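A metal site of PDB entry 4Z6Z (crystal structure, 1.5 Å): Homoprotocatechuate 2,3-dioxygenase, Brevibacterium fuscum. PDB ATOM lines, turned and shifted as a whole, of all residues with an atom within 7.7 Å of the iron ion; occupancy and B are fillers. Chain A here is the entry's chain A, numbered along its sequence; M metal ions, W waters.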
ATOM      1  N   ASP A 154       7.159   5.766   7.212  1.00  0.00           N
ATOM      2  CA  ASP A 154       6.599   7.112   7.189  1.00  0.00           C
ATOM      3  C   ASP A 154       6.443   7.773   8.554  1.00  0.00           C
ATOM      4  O   ASP A 154       6.822   8.947   8.707  1.00  0.00           O
ATOM      5  CB  ASP A 154       5.261   7.206   6.452  1.00  0.00           C
ATOM      6  CG  ASP A 154       4.856   8.677   6.209  1.00  0.00           C
ATOM      7  OD1 ASP A 154       5.502   9.325   5.359  1.00  0.00           O
ATOM      8  OD2 ASP A 154       3.951   9.203   6.927  1.00  0.00           O
ATOM      9  N   HIS A 155       5.849   7.078   9.520  1.00  0.00           N
ATOM     10  CA  HIS A 155       5.530   7.706  10.817  1.00  0.00           C
ATOM     11  C   HIS A 155       5.205   6.736  11.916  1.00  0.00           C
ATOM     12  O   HIS A 155       4.975   5.566  11.671  1.00  0.00           O
ATOM     13  CB  HIS A 155       4.375   8.705  10.676  1.00  0.00           C
ATOM     14  CG  HIS A 155       3.059   8.093  10.326  1.00  0.00           C
ATOM     15  ND1 HIS A 155       2.604   8.025   9.026  1.00  0.00           N
ATOM     16  CD2 HIS A 155       2.083   7.560  11.087  1.00  0.00           C
ATOM     17  CE1 HIS A 155       1.399   7.488   9.005  1.00  0.00           C
ATOM     18  NE2 HIS A 155       1.056   7.191  10.242  1.00  0.00           N
ATOM     19  N   PHE A 156       5.178   7.255  13.147  1.00  0.00           N
ATOM     20  CA  PHE A 156       4.644   6.606  14.310  1.00  0.00           C
ATOM     21  C   PHE A 156       3.355   7.322  14.716  1.00  0.00           C
ATOM     22  O   PHE A 156       3.122   8.480  14.358  1.00  0.00           O
ATOM     23  CB  PHE A 156       5.626   6.685  15.491  1.00  0.00           C
ATOM     24  CG  PHE A 156       7.058   6.310  15.153  1.00  0.00           C
ATOM     25  CD1 PHE A 156       7.369   5.062  14.628  1.00  0.00           C
ATOM     26  CD2 PHE A 156       8.102   7.207  15.392  1.00  0.00           C
ATOM     27  CE1 PHE A 156       8.679   4.720  14.352  1.00  0.00           C
ATOM     28  CE2 PHE A 156       9.413   6.865  15.115  1.00  0.00           C
ATOM     29  CZ  PHE A 156       9.708   5.630  14.592  1.00  0.00           C
ATOM     30  N   ASN A 157       2.527   6.636  15.486  1.00  0.00           N
ATOM     31  CA  ASN A 157       1.377   7.269  16.129  1.00  0.00           C
ATOM     32  C   ASN A 157       1.277   6.766  17.574  1.00  0.00           C
ATOM     33  O   ASN A 157       1.224   5.577  17.806  1.00  0.00           O
ATOM     34  CB  ASN A 157       0.113   6.969  15.325  1.00  0.00           C
ATOM     35  CG  ASN A 157      -1.095   7.724  15.836  1.00  0.00           C
ATOM     36  OD1 ASN A 157      -1.505   7.548  16.982  1.00  0.00           O
ATOM     37  ND2 ASN A 157      -1.695   8.544  14.987  1.00  0.00           N
ATOM     38  N   TRP A 192      -1.143  15.891  14.543  1.00  0.00           N
ATOM     39  CA  TRP A 192      -0.145  15.360  13.645  1.00  0.00           C
ATOM     40  C   TRP A 192       1.011  16.344  13.541  1.00  0.00           C
ATOM     41  O   TRP A 192       0.769  17.532  13.352  1.00  0.00           O
ATOM     42  CB  TRP A 192      -0.759  15.156  12.256  1.00  0.00           C
ATOM     43  CG  TRP A 192      -1.673  13.958  12.137  1.00  0.00           C
ATOM     44  CD1 TRP A 192      -1.389  12.785  11.513  1.00  0.00           C
ATOM     45  CD2 TRP A 192      -3.010  13.826  12.631  1.00  0.00           C
ATOM     46  NE1 TRP A 192      -2.440  11.916  11.597  1.00  0.00           N
ATOM     47  CE2 TRP A 192      -3.462  12.528  12.264  1.00  0.00           C
ATOM     48  CE3 TRP A 192      -3.885  14.678  13.327  1.00  0.00           C
ATOM     49  CZ2 TRP A 192      -4.737  12.050  12.599  1.00  0.00           C
ATOM     50  CZ3 TRP A 192      -5.158  14.187  13.659  1.00  0.00           C
ATOM     51  CH2 TRP A 192      -5.566  12.881  13.282  1.00  0.00           C
ATOM     52  N   HIS A 200       3.398  13.965   8.746  1.00  0.00           N
ATOM     53  CA  HIS A 200       3.925  13.659  10.065  1.00  0.00           C
ATOM     54  C   HIS A 200       5.086  12.696  10.101  1.00  0.00           C
ATOM     55  O   HIS A 200       5.270  11.885   9.178  1.00  0.00           O
ATOM     56  CB  HIS A 200       2.845  13.222  11.055  1.00  0.00           C
ATOM     57  CG  HIS A 200       1.994  12.043  10.657  1.00  0.00           C
ATOM     58  ND1 HIS A 200       1.545  11.803   9.383  1.00  0.00           N
ATOM     59  CD2 HIS A 200       1.445  11.078  11.437  1.00  0.00           C
ATOM     60  CE1 HIS A 200       0.752  10.739   9.381  1.00  0.00           C
ATOM     61  NE2 HIS A 200       0.678  10.294  10.624  1.00  0.00           N
ATOM     62  N   ALA A 203       2.517  11.312  15.652  1.00  0.00           N
ATOM     63  CA  ALA A 203       1.207  11.868  15.871  1.00  0.00           C
ATOM     64  C   ALA A 203       0.768  11.465  17.265  1.00  0.00           C
ATOM     65  O   ALA A 203       1.225  10.448  17.799  1.00  0.00           O
ATOM     66  CB  ALA A 203       0.222  11.356  14.825  1.00  0.00           C
ATOM     67  N   THR A 205      -2.642  10.600  19.476  1.00  0.00           N
ATOM     68  CA  THR A 205      -4.052  10.215  19.535  1.00  0.00           C
ATOM     69  C   THR A 205      -4.467  10.213  21.003  1.00  0.00           C
ATOM     70  O   THR A 205      -3.810   9.590  21.835  1.00  0.00           O
ATOM     71  CB  THR A 205      -4.236   8.798  18.955  1.00  0.00           C
ATOM     72  OG1 THR A 205      -3.785   8.784  17.589  1.00  0.00           O
ATOM     73  CG2 THR A 205      -5.704   8.322  19.043  1.00  0.00           C
ATOM     74  N   HIS A 213       0.069   3.429  19.051  1.00  0.00           N
ATOM     75  CA  HIS A 213      -1.062   3.123  18.203  1.00  0.00           C
ATOM     76  C   HIS A 213      -0.684   2.322  16.966  1.00  0.00           C
ATOM     77  O   HIS A 213      -1.257   1.257  16.711  1.00  0.00           O
ATOM     78  CB  HIS A 213      -1.842   4.379  17.800  1.00  0.00           C
ATOM     79  CG  HIS A 213      -3.223   4.065  17.334  1.00  0.00           C
ATOM     80  ND1 HIS A 213      -3.497   3.594  16.074  1.00  0.00           N
ATOM     81  CD2 HIS A 213      -4.406   4.053  17.996  1.00  0.00           C
ATOM     82  CE1 HIS A 213      -4.784   3.353  15.946  1.00  0.00           C
ATOM     83  NE2 HIS A 213      -5.366   3.615  17.100  1.00  0.00           N
ATOM     84  N   HIS A 214       0.267   2.825  16.197  1.00  0.00           N
ATOM     85  CA  HIS A 214       0.775   2.092  15.044  1.00  0.00           C
ATOM     86  C   HIS A 214       2.100   2.619  14.559  1.00  0.00           C
ATOM     87  O   HIS A 214       2.526   3.710  14.933  1.00  0.00           O
ATOM     88  CB  HIS A 214      -0.237   2.101  13.879  1.00  0.00           C
ATOM     89  CG  HIS A 214      -0.615   3.479  13.394  1.00  0.00           C
ATOM     90  ND1 HIS A 214      -1.701   4.162  13.888  1.00  0.00           N
ATOM     91  CD2 HIS A 214      -0.078   4.262  12.432  1.00  0.00           C
ATOM     92  CE1 HIS A 214      -1.807   5.319  13.271  1.00  0.00           C
ATOM     93  NE2 HIS A 214      -0.847   5.406  12.376  1.00  0.00           N
ATOM     94  N   VAL A 215       2.720   1.812  13.693  1.00  0.00           N
ATOM     95  CA  VAL A 215       3.812   2.229  12.844  1.00  0.00           C
ATOM     96  C   VAL A 215       3.333   2.182  11.393  1.00  0.00           C
ATOM     97  O   VAL A 215       2.593   1.261  11.025  1.00  0.00           O
ATOM     98  CB  VAL A 215       5.024   1.275  13.038  1.00  0.00           C
ATOM     99  CG1 VAL A 215       6.152   1.668  12.114  1.00  0.00           C
ATOM    100  CG2 VAL A 215       5.498   1.300  14.494  1.00  0.00           C
ATOM    101  N   ALA A 216       3.718   3.171  10.588  1.00  0.00           N
ATOM    102  CA  ALA A 216       3.261   3.283   9.222  1.00  0.00           C
ATOM    103  C   ALA A 216       4.395   3.187   8.208  1.00  0.00           C
ATOM    104  O   ALA A 216       5.408   3.887   8.333  1.00  0.00           O
ATOM    105  CB  ALA A 216       2.498   4.582   9.014  1.00  0.00           C
ATOM    106  N   HIS A 248      -7.875   8.901   3.850  1.00  0.00           N
ATOM    107  CA  HIS A 248      -7.960   9.698   5.073  1.00  0.00           C
ATOM    108  C   HIS A 248      -8.496  11.115   4.749  1.00  0.00           C
ATOM    109  O   HIS A 248      -8.223  11.671   3.664  1.00  0.00           O
ATOM    110  CB  HIS A 248      -6.565   9.864   5.704  1.00  0.00           C
ATOM    111  CG  HIS A 248      -6.112   8.708   6.526  1.00  0.00           C
ATOM    112  ND1 HIS A 248      -6.881   8.129   7.515  1.00  0.00           N
ATOM    113  CD2 HIS A 248      -4.915   8.075   6.561  1.00  0.00           C
ATOM    114  CE1 HIS A 248      -6.190   7.169   8.096  1.00  0.00           C
ATOM    115  NE2 HIS A 248      -4.996   7.116   7.544  1.00  0.00           N
ATOM    116  N   SER A 251      -4.627  14.343   6.563  1.00  0.00           N
ATOM    117  CA  SER A 251      -3.452  13.867   5.800  1.00  0.00           C
ATOM    118  C   SER A 251      -3.706  13.625   4.313  1.00  0.00           C
ATOM    119  O   SER A 251      -2.756  13.655   3.518  1.00  0.00           O
ATOM    120  CB  SER A 251      -2.801  12.601   6.407  1.00  0.00           C
ATOM    121  OG  SER A 251      -3.419  11.413   5.950  1.00  0.00           O
ATOM    122  N   TYR A 255      -4.897   4.660   2.676  1.00  0.00           N
ATOM    123  CA  TYR A 255      -4.476   3.952   3.885  1.00  0.00           C
ATOM    124  C   TYR A 255      -5.084   2.568   4.053  1.00  0.00           C
ATOM    125  O   TYR A 255      -6.114   2.242   3.462  1.00  0.00           O
ATOM    126  CB  TYR A 255      -4.766   4.780   5.143  1.00  0.00           C
ATOM    127  CG  TYR A 255      -6.227   4.766   5.531  1.00  0.00           C
ATOM    128  CD1 TYR A 255      -6.755   3.774   6.348  1.00  0.00           C
ATOM    129  CD2 TYR A 255      -7.081   5.777   5.084  1.00  0.00           C
ATOM    130  CE1 TYR A 255      -8.091   3.757   6.702  1.00  0.00           C
ATOM    131  CE2 TYR A 255      -8.432   5.777   5.421  1.00  0.00           C
ATOM    132  CZ  TYR A 255      -8.929   4.777   6.217  1.00  0.00           C
ATOM    133  OH  TYR A 255     -10.259   4.768   6.574  1.00  0.00           O
ATOM    134  N   LEU A 256      -4.425   1.786   4.924  1.00  0.00           N
ATOM    135  CA  LEU A 256      -4.900   0.493   5.385  1.00  0.00           C
ATOM    136  C   LEU A 256      -4.293   0.217   6.746  1.00  0.00           C
ATOM    137  O   LEU A 256      -3.126   0.538   6.955  1.00  0.00           O
ATOM    138  CB  LEU A 256      -4.431  -0.578   4.385  1.00  0.00           C
ATOM    139  CG  LEU A 256      -4.694  -2.028   4.765  1.00  0.00           C
ATOM    140  CD1 LEU A 256      -6.183  -2.306   4.718  1.00  0.00           C
ATOM    141  CD2 LEU A 256      -3.895  -2.977   3.861  1.00  0.00           C
ATOM    142  N   TYR A 257      -5.067  -0.390   7.648  1.00  0.00           N
ATOM    143  CA  TYR A 257      -4.554  -0.853   8.954  1.00  0.00           C
ATOM    144  C   TYR A 257      -4.722  -2.362   9.093  1.00  0.00           C
ATOM    145  O   TYR A 257      -5.830  -2.901   8.914  1.00  0.00           O
ATOM    146  CB  TYR A 257      -5.287  -0.176  10.123  1.00  0.00           C
ATOM    147  CG  TYR A 257      -5.161   1.322  10.164  1.00  0.00           C
ATOM    148  CD1 TYR A 257      -4.095   1.940  10.796  1.00  0.00           C
ATOM    149  CD2 TYR A 257      -6.129   2.116   9.583  1.00  0.00           C
ATOM    150  CE1 TYR A 257      -3.989   3.334  10.835  1.00  0.00           C
ATOM    151  CE2 TYR A 257      -6.034   3.497   9.608  1.00  0.00           C
ATOM    152  CZ  TYR A 257      -4.968   4.100  10.248  1.00  0.00           C
ATOM    153  OH  TYR A 257      -4.899   5.451  10.265  1.00  0.00           O
ATOM    154  N   GLU A 267       0.132   0.459   9.778  1.00  0.00           N
ATOM    155  CA  GLU A 267      -0.545   1.199   8.713  1.00  0.00           C
ATOM    156  C   GLU A 267       0.266   1.139   7.430  1.00  0.00           C
ATOM    157  O   GLU A 267       1.491   1.288   7.444  1.00  0.00           O
ATOM    158  CB  GLU A 267      -0.742   2.668   9.096  1.00  0.00           C
ATOM    159  CG  GLU A 267      -1.661   3.414   8.130  1.00  0.00           C
ATOM    160  CD  GLU A 267      -1.835   4.883   8.484  1.00  0.00           C
ATOM    161  OE1 GLU A 267      -1.147   5.317   9.413  1.00  0.00           O
ATOM    162  OE2 GLU A 267      -2.628   5.600   7.837  1.00  0.00           O
ATOM    163  N   ILE A 268      -0.435   0.969   6.299  1.00  0.00           N
ATOM    164  CA  ILE A 268       0.152   1.225   4.986  1.00  0.00           C
ATOM    165  C   ILE A 268      -0.472   2.488   4.411  1.00  0.00           C
ATOM    166  O   ILE A 268      -1.688   2.697   4.533  1.00  0.00           O
ATOM    167  CB  ILE A 268      -0.064   0.060   4.006  1.00  0.00           C
ATOM    168  CG1 ILE A 268      -0.001  -1.317   4.687  1.00  0.00           C
ATOM    169  CG2 ILE A 268       0.924   0.134   2.865  1.00  0.00           C
ATOM    170  CD1 ILE A 268       1.320  -1.626   5.338  1.00  0.00           C
ATOM    171  N   TYR A 269       0.344   3.370   3.855  1.00  0.00           N
ATOM    172  CA  TYR A 269       0.003   4.800   3.669  1.00  0.00           C
ATOM    173  C   TYR A 269       0.597   5.302   2.367  1.00  0.00           C
ATOM    174  O   TYR A 269       1.696   4.917   2.017  1.00  0.00           O
ATOM    175  CB  TYR A 269       0.617   5.522   4.858  1.00  0.00           C
ATOM    176  CG  TYR A 269       0.476   7.005   5.054  1.00  0.00           C
ATOM    177  CD1 TYR A 269      -0.521   7.516   5.875  1.00  0.00           C
ATOM    178  CD2 TYR A 269       1.425   7.887   4.527  1.00  0.00           C
ATOM    179  CE1 TYR A 269      -0.600   8.877   6.131  1.00  0.00           C
ATOM    180  CE2 TYR A 269       1.359   9.261   4.796  1.00  0.00           C
ATOM    181  CZ  TYR A 269       0.323   9.745   5.589  1.00  0.00           C
ATOM    182  OH  TYR A 269       0.236  11.089   5.892  1.00  0.00           O
ATOM    183  N   ARG A 293     -11.663  11.141   9.328  1.00  0.00           N
ATOM    184  CA  ARG A 293     -10.768   9.987   9.421  1.00  0.00           C
ATOM    185  C   ARG A 293     -10.812   9.129   8.187  1.00  0.00           C
ATOM    186  O   ARG A 293      -9.771   8.743   7.670  1.00  0.00           O
ATOM    187  CB  ARG A 293     -11.062   9.177  10.678  1.00  0.00           C
ATOM    188  CG  ARG A 293     -10.665   9.940  11.954  1.00  0.00           C
ATOM    189  CD  ARG A 293     -10.293   9.023  13.097  1.00  0.00           C
ATOM    190  NE  ARG A 293      -9.775   9.705  14.292  1.00  0.00           N
ATOM    191  CZ  ARG A 293      -8.492   9.939  14.562  1.00  0.00           C
ATOM    192  NH1 ARG A 293      -7.543   9.593  13.731  1.00  0.00           N
ATOM    193  NH2 ARG A 293      -8.161  10.512  15.703  1.00  0.00           N
ATOM    194  N   TRP A 304     -10.169   0.226  16.740  1.00  0.00           N
ATOM    195  CA  TRP A 304      -9.169   1.193  16.285  1.00  0.00           C
ATOM    196  C   TRP A 304      -8.953   2.288  17.333  1.00  0.00           C
ATOM    197  O   TRP A 304      -7.848   2.794  17.494  1.00  0.00           O
ATOM    198  CB  TRP A 304      -9.579   1.758  14.924  1.00  0.00           C
ATOM    199  CG  TRP A 304      -8.460   2.457  14.237  1.00  0.00           C
ATOM    200  CD1 TRP A 304      -7.569   1.902  13.369  1.00  0.00           C
ATOM    201  CD2 TRP A 304      -8.116   3.830  14.357  1.00  0.00           C
ATOM    202  NE1 TRP A 304      -6.670   2.850  12.955  1.00  0.00           N
ATOM    203  CE2 TRP A 304      -6.980   4.042  13.540  1.00  0.00           C
ATOM    204  CE3 TRP A 304      -8.640   4.903  15.068  1.00  0.00           C
ATOM    205  CZ2 TRP A 304      -6.366   5.300  13.428  1.00  0.00           C
ATOM    206  CZ3 TRP A 304      -8.038   6.130  14.960  1.00  0.00           C
ATOM    207  CH2 TRP A 304      -6.902   6.325  14.159  1.00  0.00           C
HETATM  208 FE    FE M   1      -1.078   6.874  10.752  1.00  0.00          FE
HETATM  209  O   HOH W   1      -0.933   8.626  12.176  1.00  0.00           O
HETATM  210  O   HOH W   2      -1.630   8.240   9.230  1.00  0.00           O
HETATM  211  O   HOH W   3      -3.212   7.005  11.129  1.00  0.00           O
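O of His 155 lies within hydrogen-bond range of N of Ala 216 (2.9 Å). The side-chain carboxylate (OE2) of Glu 267 is in hydrogen-bond range of the side-chain hydroxyl (OH) of Tyr 257 (3.3 Å). The side-chain carboxylate (OE2) of Glu 267 sits at hydrogen-bond distance from a ring nitrogen (NE2) of His 248. The side-chain carboxylate of Asp 154 is in hydrogen-bond range of a ring nitrogen (ND1) of His 155 (2.8 Å). A ring nitrogen (NE2) of His 200 lies close to a ring nitrogen (ND1) of His 155 (3.4 Å). A ring nitrogen (ND1) of His 214 sits at hydrogen-bond distance from a ring nitrogen (ND1) of His 213, 2.9 Å away. The backbone carbonyl oxygen (O) of His 214 lies within hydrogen-bond range of the backbone NH (N) of Asn 157, at 3.0 Å. The backbone NH (N) of Glu 267 lies within hydrogen-bond range of the backbone carbonyl oxygen (O) of Val 215, 2.9 Å away.
The iron ion is bound by OE1 of Glu 267, at 2.1 Å. Water W2 is bound to the iron ion, 2.1 Å away. Water W3 is bound to the iron ion, 2.2 Å away. NE2 of His 214 binds the iron ion. NE2 of His 155 binds the iron ion, at 2.2 Å. The iron ion is bound by water W1, at 2.3 Å. The iron ion has six donor atoms within binding distance.
Water W1 lies within hydrogen-bond range of NE2 of His 200 (2.8 Å) and ND2 of Asn 157 (2.9 Å). Water W2 bridges the side-chain carboxylate (OE2) of Glu 267 (3.1 Å) and a ring nitrogen (NE2) of His 200 (3.4 Å).
His 200 touches the iron ion (NE2 to FE, 3.8 Å). Of the 22 residues printed, 4 come within 4 Å of the iron ion. Along chain A the residues within 4 Å of the iron ion span positions 155 to 267. The nearest printed residue that does not touch the iron ion is Tyr 257 (4.1 Å).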
